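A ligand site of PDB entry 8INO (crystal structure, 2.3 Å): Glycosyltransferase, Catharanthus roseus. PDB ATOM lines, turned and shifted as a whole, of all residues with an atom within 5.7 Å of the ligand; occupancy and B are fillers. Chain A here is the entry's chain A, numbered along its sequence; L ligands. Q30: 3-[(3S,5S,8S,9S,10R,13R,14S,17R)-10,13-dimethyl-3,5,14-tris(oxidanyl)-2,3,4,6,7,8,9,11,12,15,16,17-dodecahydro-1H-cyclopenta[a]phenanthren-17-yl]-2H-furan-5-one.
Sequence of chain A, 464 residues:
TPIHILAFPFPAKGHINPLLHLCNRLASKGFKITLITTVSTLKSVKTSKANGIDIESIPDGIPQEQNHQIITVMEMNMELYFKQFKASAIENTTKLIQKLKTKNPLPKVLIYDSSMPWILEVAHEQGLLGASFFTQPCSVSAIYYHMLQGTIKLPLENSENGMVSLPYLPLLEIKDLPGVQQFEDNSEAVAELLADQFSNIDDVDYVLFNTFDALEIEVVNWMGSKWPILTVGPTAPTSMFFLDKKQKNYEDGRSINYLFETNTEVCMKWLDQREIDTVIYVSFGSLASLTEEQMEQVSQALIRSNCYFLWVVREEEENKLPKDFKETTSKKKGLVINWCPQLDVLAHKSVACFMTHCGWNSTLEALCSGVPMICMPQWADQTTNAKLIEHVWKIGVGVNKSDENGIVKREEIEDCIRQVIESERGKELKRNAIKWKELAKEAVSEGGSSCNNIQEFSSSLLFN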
ATOM      1  N   PHE A  10     -15.153 -14.672   1.144  1.00  0.00           N
ATOM      2  CA  PHE A  10     -15.083 -14.574  -0.308  1.00  0.00           C
ATOM      3  C   PHE A  10     -14.585 -15.905  -0.876  1.00  0.00           C
ATOM      4  O   PHE A  10     -13.661 -16.509  -0.313  1.00  0.00           O
ATOM      5  CB  PHE A  10     -14.162 -13.427  -0.726  1.00  0.00           C
ATOM      6  CG  PHE A  10     -14.256 -13.119  -2.187  1.00  0.00           C
ATOM      7  CD1 PHE A  10     -15.326 -12.395  -2.695  1.00  0.00           C
ATOM      8  CD2 PHE A  10     -13.312 -13.587  -3.062  1.00  0.00           C
ATOM      9  CE1 PHE A  10     -15.431 -12.112  -4.039  1.00  0.00           C
ATOM     10  CE2 PHE A  10     -13.410 -13.313  -4.428  1.00  0.00           C
ATOM     11  CZ  PHE A  10     -14.475 -12.577  -4.902  1.00  0.00           C
ATOM     12  N   ALA A  12     -12.351 -17.631  -2.482  1.00  0.00           N
ATOM     13  CA  ALA A  12     -11.005 -17.840  -2.998  1.00  0.00           C
ATOM     14  C   ALA A  12     -10.137 -18.258  -1.824  1.00  0.00           C
ATOM     15  O   ALA A  12     -10.365 -17.827  -0.690  1.00  0.00           O
ATOM     16  CB  ALA A  12     -10.423 -16.601  -3.693  1.00  0.00           C
ATOM     17  N   HIS A  15      -8.905 -16.104   0.924  1.00  0.00           N
ATOM     18  CA  HIS A  15      -9.919 -15.595   1.832  1.00  0.00           C
ATOM     19  C   HIS A  15     -10.542 -16.691   2.678  1.00  0.00           C
ATOM     20  O   HIS A  15     -10.803 -16.481   3.863  1.00  0.00           O
ATOM     21  CB  HIS A  15     -11.013 -14.876   1.034  1.00  0.00           C
ATOM     22  CG  HIS A  15     -10.523 -13.680   0.260  1.00  0.00           C
ATOM     23  ND1 HIS A  15     -10.767 -12.383   0.658  1.00  0.00           N
ATOM     24  CD2 HIS A  15      -9.803 -13.595  -0.882  1.00  0.00           C
ATOM     25  CE1 HIS A  15     -10.238 -11.553  -0.214  1.00  0.00           C
ATOM     26  NE2 HIS A  15      -9.646 -12.262  -1.161  1.00  0.00           N
ATOM     27  N   MET A  74     -15.162 -14.626 -13.036  1.00  0.00           N
ATOM     28  CA  MET A  74     -15.393 -13.243 -12.649  1.00  0.00           C
ATOM     29  C   MET A  74     -14.514 -12.259 -13.405  1.00  0.00           C
ATOM     30  O   MET A  74     -14.867 -11.075 -13.483  1.00  0.00           O
ATOM     31  CB  MET A  74     -15.188 -13.076 -11.146  1.00  0.00           C
ATOM     32  CG  MET A  74     -16.359 -12.449 -10.461  1.00  0.00           C
ATOM     33  SD  MET A  74     -16.115 -12.319  -8.695  1.00  0.00           S
ATOM     34  CE  MET A  74     -16.453 -14.005  -8.181  1.00  0.00           C
ATOM     35  N   GLU A  75     -13.386 -12.696 -13.949  1.00  0.00           N
ATOM     36  CA  GLU A  75     -12.488 -11.747 -14.598  1.00  0.00           C
ATOM     37  C   GLU A  75     -12.948 -11.357 -15.990  1.00  0.00           C
ATOM     38  O   GLU A  75     -12.515 -10.307 -16.493  1.00  0.00           O
ATOM     39  CB  GLU A  75     -11.085 -12.331 -14.678  1.00  0.00           C
ATOM     40  CG  GLU A  75     -10.995 -13.610 -15.476  1.00  0.00           C
ATOM     41  CD  GLU A  75      -9.720 -13.673 -16.284  1.00  0.00           C
ATOM     42  OE1 GLU A  75      -8.926 -14.606 -16.051  1.00  0.00           O
ATOM     43  OE2 GLU A  75      -9.525 -12.790 -17.152  1.00  0.00           O
ATOM     44  N   MET A  78     -15.635  -7.935 -14.626  1.00  0.00           N
ATOM     45  CA  MET A  78     -15.650  -7.812 -13.172  1.00  0.00           C
ATOM     46  C   MET A  78     -16.887  -7.050 -12.699  1.00  0.00           C
ATOM     47  O   MET A  78     -17.544  -7.465 -11.747  1.00  0.00           O
ATOM     48  CB  MET A  78     -14.381  -7.123 -12.675  1.00  0.00           C
ATOM     49  CG  MET A  78     -14.320  -6.969 -11.156  1.00  0.00           C
ATOM     50  SD  MET A  78     -14.029  -8.556 -10.350  1.00  0.00           S
ATOM     51  CE  MET A  78     -12.457  -8.956 -11.115  1.00  0.00           C
ATOM     52  N   ASP A 113     -16.405 -11.865   4.932  1.00  0.00           N
ATOM     53  CA  ASP A 113     -15.223 -11.260   4.334  1.00  0.00           C
ATOM     54  C   ASP A 113     -15.442  -9.763   4.121  1.00  0.00           C
ATOM     55  O   ASP A 113     -16.460  -9.346   3.570  1.00  0.00           O
ATOM     56  CB  ASP A 113     -14.918 -11.961   3.014  1.00  0.00           C
ATOM     57  CG  ASP A 113     -13.580 -11.560   2.457  1.00  0.00           C
ATOM     58  OD1 ASP A 113     -13.456 -10.450   1.890  1.00  0.00           O
ATOM     59  OD2 ASP A 113     -12.643 -12.376   2.574  1.00  0.00           O
ATOM     60  N   SER A 114     -14.442  -8.966   4.526  1.00  0.00           N
ATOM     61  CA  SER A 114     -14.527  -7.509   4.438  1.00  0.00           C
ATOM     62  C   SER A 114     -14.814  -7.008   3.034  1.00  0.00           C
ATOM     63  O   SER A 114     -15.271  -5.872   2.875  1.00  0.00           O
ATOM     64  CB  SER A 114     -13.231  -6.861   4.928  1.00  0.00           C
ATOM     65  OG  SER A 114     -12.174  -7.070   3.987  1.00  0.00           O
ATOM     66  N   SER A 115     -14.513  -7.802   2.002  1.00  0.00           N
ATOM     67  CA  SER A 115     -14.792  -7.389   0.630  1.00  0.00           C
ATOM     68  C   SER A 115     -16.262  -7.550   0.273  1.00  0.00           C
ATOM     69  O   SER A 115     -16.646  -7.212  -0.857  1.00  0.00           O
ATOM     70  CB  SER A 115     -13.937  -8.193  -0.347  1.00  0.00           C
ATOM     71  OG  SER A 115     -14.347  -9.569  -0.336  1.00  0.00           O
ATOM     72  N   THR A 135      -8.807  -9.523   5.411  1.00  0.00           N
ATOM     73  CA  THR A 135      -7.749 -10.496   5.134  1.00  0.00           C
ATOM     74  C   THR A 135      -6.458  -9.860   4.634  1.00  0.00           C
ATOM     75  O   THR A 135      -5.592 -10.581   4.139  1.00  0.00           O
ATOM     76  CB  THR A 135      -8.239 -11.499   4.100  1.00  0.00           C
ATOM     77  OG1 THR A 135      -8.605 -10.788   2.910  1.00  0.00           O
ATOM     78  CG2 THR A 135      -9.420 -12.266   4.642  1.00  0.00           C
ATOM     79  N   GLN A 136      -6.340  -8.543   4.698  1.00  0.00           N
ATOM     80  CA  GLN A 136      -5.138  -7.804   4.367  1.00  0.00           C
ATOM     81  C   GLN A 136      -4.757  -6.998   5.605  1.00  0.00           C
ATOM     82  O   GLN A 136      -5.627  -6.726   6.443  1.00  0.00           O
ATOM     83  CB  GLN A 136      -5.363  -6.871   3.166  1.00  0.00           C
ATOM     84  CG  GLN A 136      -5.452  -7.589   1.829  1.00  0.00           C
ATOM     85  CD  GLN A 136      -5.942  -6.702   0.698  1.00  0.00           C
ATOM     86  OE1 GLN A 136      -5.297  -5.712   0.324  1.00  0.00           O
ATOM     87  NE2 GLN A 136      -7.098  -7.049   0.153  1.00  0.00           N
ATOM     88  N   TYR A 144      -7.185   1.613   1.074  1.00  0.00           N
ATOM     89  CA  TYR A 144      -8.552   1.522   0.587  1.00  0.00           C
ATOM     90  C   TYR A 144      -9.445   2.561   1.263  1.00  0.00           C
ATOM     91  O   TYR A 144     -10.283   3.190   0.600  1.00  0.00           O
ATOM     92  CB  TYR A 144      -9.086   0.106   0.816  1.00  0.00           C
ATOM     93  CG  TYR A 144      -8.178  -0.949   0.220  1.00  0.00           C
ATOM     94  CD1 TYR A 144      -7.372  -0.673  -0.894  1.00  0.00           C
ATOM     95  CD2 TYR A 144      -8.110  -2.228   0.766  1.00  0.00           C
ATOM     96  CE1 TYR A 144      -6.516  -1.641  -1.444  1.00  0.00           C
ATOM     97  CE2 TYR A 144      -7.277  -3.200   0.223  1.00  0.00           C
ATOM     98  CZ  TYR A 144      -6.496  -2.905  -0.888  1.00  0.00           C
ATOM     99  OH  TYR A 144      -5.668  -3.890  -1.414  1.00  0.00           O
ATOM    100  N   PHE A 183      -5.380  -5.034 -14.104  1.00  0.00           N
ATOM    101  CA  PHE A 183      -6.666  -5.630 -14.469  1.00  0.00           C
ATOM    102  C   PHE A 183      -7.336  -4.927 -15.636  1.00  0.00           C
ATOM    103  O   PHE A 183      -8.479  -5.268 -15.963  1.00  0.00           O
ATOM    104  CB  PHE A 183      -7.594  -5.642 -13.246  1.00  0.00           C
ATOM    105  CG  PHE A 183      -7.004  -6.330 -12.052  1.00  0.00           C
ATOM    106  CD1 PHE A 183      -6.484  -7.609 -12.166  1.00  0.00           C
ATOM    107  CD2 PHE A 183      -6.933  -5.685 -10.836  1.00  0.00           C
ATOM    108  CE1 PHE A 183      -5.926  -8.239 -11.065  1.00  0.00           C
ATOM    109  CE2 PHE A 183      -6.383  -6.312  -9.735  1.00  0.00           C
ATOM    110  CZ  PHE A 183      -5.873  -7.586  -9.848  1.00  0.00           C
ATOM    111  N   ASN A 186     -11.208  -4.256 -16.129  1.00  0.00           N
ATOM    112  CA  ASN A 186     -11.666  -4.467 -14.765  1.00  0.00           C
ATOM    113  C   ASN A 186     -11.021  -3.533 -13.744  1.00  0.00           C
ATOM    114  O   ASN A 186     -11.385  -3.587 -12.575  1.00  0.00           O
ATOM    115  CB  ASN A 186     -11.417  -5.916 -14.354  1.00  0.00           C
ATOM    116  CG  ASN A 186     -12.132  -6.889 -15.246  1.00  0.00           C
ATOM    117  OD1 ASN A 186     -13.224  -6.605 -15.719  1.00  0.00           O
ATOM    118  ND2 ASN A 186     -11.521  -8.043 -15.468  1.00  0.00           N
ATOM    119  N   VAL A 190     -12.419  -3.076  -9.859  1.00  0.00           N
ATOM    120  CA  VAL A 190     -11.622  -3.592  -8.754  1.00  0.00           C
ATOM    121  C   VAL A 190     -11.308  -2.489  -7.755  1.00  0.00           C
ATOM    122  O   VAL A 190     -11.317  -2.706  -6.539  1.00  0.00           O
ATOM    123  CB  VAL A 190     -10.344  -4.277  -9.288  1.00  0.00           C
ATOM    124  CG1 VAL A 190      -9.435  -4.726  -8.137  1.00  0.00           C
ATOM    125  CG2 VAL A 190     -10.704  -5.469 -10.167  1.00  0.00           C
ATOM    126  N   LEU A 194     -12.408  -2.506  -3.640  1.00  0.00           N
ATOM    127  CA  LEU A 194     -11.483  -2.337  -2.516  1.00  0.00           C
ATOM    128  C   LEU A 194     -11.896  -1.172  -1.638  1.00  0.00           C
ATOM    129  O   LEU A 194     -11.913  -1.300  -0.414  1.00  0.00           O
ATOM    130  CB  LEU A 194     -10.055  -2.145  -3.040  1.00  0.00           C
ATOM    131  CG  LEU A 194      -9.445  -3.358  -3.768  1.00  0.00           C
ATOM    132  CD1 LEU A 194      -8.242  -2.919  -4.575  1.00  0.00           C
ATOM    133  CD2 LEU A 194      -9.068  -4.451  -2.784  1.00  0.00           C
ATOM    134  N   GLN A 197     -14.884  -1.647   0.888  1.00  0.00           N
ATOM    135  CA  GLN A 197     -14.707  -2.376   2.141  1.00  0.00           C
ATOM    136  C   GLN A 197     -14.921  -1.496   3.354  1.00  0.00           C
ATOM    137  O   GLN A 197     -15.168  -2.017   4.440  1.00  0.00           O
ATOM    138  CB  GLN A 197     -13.318  -2.997   2.185  1.00  0.00           C
ATOM    139  CG  GLN A 197     -13.110  -4.165   1.247  1.00  0.00           C
ATOM    140  CD  GLN A 197     -11.729  -4.805   1.420  1.00  0.00           C
ATOM    141  OE1 GLN A 197     -11.387  -5.278   2.496  1.00  0.00           O
ATOM    142  NE2 GLN A 197     -10.931  -4.797   0.370  1.00  0.00           N
ATOM    143  N   LEU A 287      -4.126 -17.851  -7.188  1.00  0.00           N
ATOM    144  CA  LEU A 287      -4.711 -17.232  -8.376  1.00  0.00           C
ATOM    145  C   LEU A 287      -3.716 -16.803  -9.429  1.00  0.00           C
ATOM    146  O   LEU A 287      -3.965 -17.025 -10.609  1.00  0.00           O
ATOM    147  CB  LEU A 287      -5.577 -16.017  -7.998  1.00  0.00           C
ATOM    148  CG  LEU A 287      -6.621 -16.242  -6.935  1.00  0.00           C
ATOM    149  CD1 LEU A 287      -6.890 -14.984  -6.086  1.00  0.00           C
ATOM    150  CD2 LEU A 287      -7.886 -16.728  -7.634  1.00  0.00           C
ATOM    151  N   ALA A 288      -2.596 -16.192  -9.045  1.00  0.00           N
ATOM    152  CA  ALA A 288      -1.702 -15.581 -10.005  1.00  0.00           C
ATOM    153  C   ALA A 288      -1.221 -16.600 -11.041  1.00  0.00           C
ATOM    154  O   ALA A 288      -0.891 -17.732 -10.696  1.00  0.00           O
ATOM    155  CB  ALA A 288      -0.525 -14.935  -9.279  1.00  0.00           C
ATOM    156  N   TRP A 379       0.096  -8.443  -8.640  1.00  0.00           N
ATOM    157  CA  TRP A 379      -0.907  -7.383  -8.750  1.00  0.00           C
ATOM    158  C   TRP A 379      -1.642  -7.232  -7.424  1.00  0.00           C
ATOM    159  O   TRP A 379      -1.334  -7.902  -6.435  1.00  0.00           O
ATOM    160  CB  TRP A 379      -1.884  -7.657  -9.901  1.00  0.00           C
ATOM    161  CG  TRP A 379      -2.111  -9.113 -10.118  1.00  0.00           C
ATOM    162  CD1 TRP A 379      -1.550  -9.902 -11.096  1.00  0.00           C
ATOM    163  CD2 TRP A 379      -2.943  -9.977  -9.341  1.00  0.00           C
ATOM    164  NE1 TRP A 379      -1.996 -11.205 -10.969  1.00  0.00           N
ATOM    165  CE2 TRP A 379      -2.859 -11.269  -9.906  1.00  0.00           C
ATOM    166  CE3 TRP A 379      -3.768  -9.782  -8.229  1.00  0.00           C
ATOM    167  CZ2 TRP A 379      -3.556 -12.364  -9.385  1.00  0.00           C
ATOM    168  CZ3 TRP A 379      -4.471 -10.862  -7.715  1.00  0.00           C
ATOM    169  CH2 TRP A 379      -4.359 -12.140  -8.284  1.00  0.00           C
ATOM    170  N   ALA A 380      -2.620  -6.331  -7.422  1.00  0.00           N
ATOM    171  CA  ALA A 380      -3.376  -5.984  -6.229  1.00  0.00           C
ATOM    172  C   ALA A 380      -2.427  -5.618  -5.091  1.00  0.00           C
ATOM    173  O   ALA A 380      -1.411  -4.944  -5.318  1.00  0.00           O
ATOM    174  CB  ALA A 380      -4.311  -7.110  -5.828  1.00  0.00           C
ATOM    175  N   ASP A 381      -2.732  -6.070  -3.881  1.00  0.00           N
ATOM    176  CA  ASP A 381      -1.974  -5.671  -2.711  1.00  0.00           C
ATOM    177  C   ASP A 381      -0.578  -6.274  -2.662  1.00  0.00           C
ATOM    178  O   ASP A 381       0.199  -5.910  -1.776  1.00  0.00           O
ATOM    179  CB  ASP A 381      -2.752  -6.041  -1.441  1.00  0.00           C
ATOM    180  CG  ASP A 381      -3.126  -7.517  -1.397  1.00  0.00           C
ATOM    181  OD1 ASP A 381      -3.676  -8.016  -2.407  1.00  0.00           O
ATOM    182  OD2 ASP A 381      -2.895  -8.189  -0.364  1.00  0.00           O
HETATM  183  C1  Q30 L   1      -9.085  -9.972 -10.884  1.00  0.00           C
HETATM  184  O1  Q30 L   1      -7.217 -14.468 -12.967  1.00  0.00           O
HETATM  185  C2  Q30 L   1      -8.673 -11.387 -10.421  1.00  0.00           C
HETATM  186  O2  Q30 L   1     -10.850 -11.791 -11.426  1.00  0.00           O
HETATM  187  C3  Q30 L   1      -7.314 -11.674 -11.086  1.00  0.00           C
HETATM  188  C4  Q30 L   1      -6.879 -13.142 -10.971  1.00  0.00           C
HETATM  189  O4  Q30 L   1      -8.695  -8.519  -1.767  1.00  0.00           O
HETATM  190  C10 Q30 L   1      -9.740 -11.701  -7.971  1.00  0.00           C
HETATM  191  C11 Q30 L   1      -8.501 -11.388  -8.855  1.00  0.00           C
HETATM  192  C12 Q30 L   1      -7.817 -10.109  -8.340  1.00  0.00           C
HETATM  193  C13 Q30 L   1      -7.856  -9.992  -6.828  1.00  0.00           C
HETATM  194  C14 Q30 L   1      -9.276  -9.777  -6.265  1.00  0.00           C
HETATM  195  C15 Q30 L   1      -9.595  -8.290  -6.150  1.00  0.00           C
HETATM  196  C16 Q30 L   1      -9.318 -10.517  -4.890  1.00  0.00           C
HETATM  197  C17 Q30 L   1      -9.397  -9.623  -3.683  1.00  0.00           C
HETATM  198  C18 Q30 L   1     -10.467  -9.231  -3.011  1.00  0.00           C
HETATM  199  C19 Q30 L   1     -10.048  -8.518  -1.811  1.00  0.00           C
HETATM  200  C20 Q30 L   1      -8.212  -8.956  -3.054  1.00  0.00           C
HETATM  201  C21 Q30 L   1     -10.495 -11.519  -4.996  1.00  0.00           C
HETATM  202  C22 Q30 L   1     -11.363 -10.940  -6.114  1.00  0.00           C
HETATM  203  C23 Q30 L   1     -10.314 -10.537  -7.148  1.00  0.00           C
HETATM  204  C5  Q30 L   1      -7.825 -14.048 -11.724  1.00  0.00           C
HETATM  205  C6  Q30 L   1      -9.110 -13.326 -12.066  1.00  0.00           C
HETATM  206  C7  Q30 L   1      -9.680 -12.477 -10.921  1.00  0.00           C
HETATM  207  C8  Q30 L   1     -10.214 -13.349  -9.792  1.00  0.00           C
HETATM  208  C9  Q30 L   1     -10.828 -12.478  -8.708  1.00  0.00           C
HETATM  209  O3  Q30 L   1     -10.689  -8.017  -0.924  1.00  0.00           O
HETATM  210  O5  Q30 L   1     -10.925  -9.599  -8.073  1.00  0.00           O
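NE2 of Gln 197 sits at hydrogen-bond distance from O3 of the ligand, at 3.5 Å.
The side-chain amide nitrogen of Gln 136 lies within hydrogen-bond range of an oxygen (O4) of the ligand (2.9 Å).
The side-chain amide oxygen (OE1) of Gln 197 sits at hydrogen-bond distance from the side-chain hydroxyl (OG) of Ser 114 (2.5 Å).
The side-chain carboxylate (OD2) of Asp 113 sits at hydrogen-bond distance from a ring nitrogen (ND1) of His 15, at 2.7 Å.
O of Glu 75 sits at hydrogen-bond distance from ND2 of Asn 186, at 2.7 Å.
OG of Ser 115 is in hydrogen-bond range of OD1 of Asp 113, at 2.6 Å.
The side-chain amide oxygen of Asn 186 is in hydrogen-bond range of the backbone NH of Met 78 (3.0 Å).
The side-chain amide oxygen (OE1) of Gln 136 is in hydrogen-bond range of the side-chain hydroxyl (OH) of Tyr 144, 2.5 Å away.
CE2 of Phe 10 touches C21 of the ligand (3.5 Å).
His 15 touches the ligand.
Glu 75 touches the ligand (CB to O2, 3.3 Å).
Met 78 touches the ligand (CE to O2, 3.3 Å).
Ser 115 touches the ligand.
CZ of Phe 183 touches C12 of the ligand, at 3.5 Å.
CZ3 of Trp 379 touches C12 of the ligand, at 3.5 Å.
Hydrophobic or aromatic side chains that line the ligand: Phe 10, His 15, Met 78, Phe 183 and Trp 379.
Nine residues have an atom within 4 Å of the ligand: Phe 10, His 15, Glu 75, Met 78, Ser 115, Gln 136, Phe 183, Gln 197 and Trp 379.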
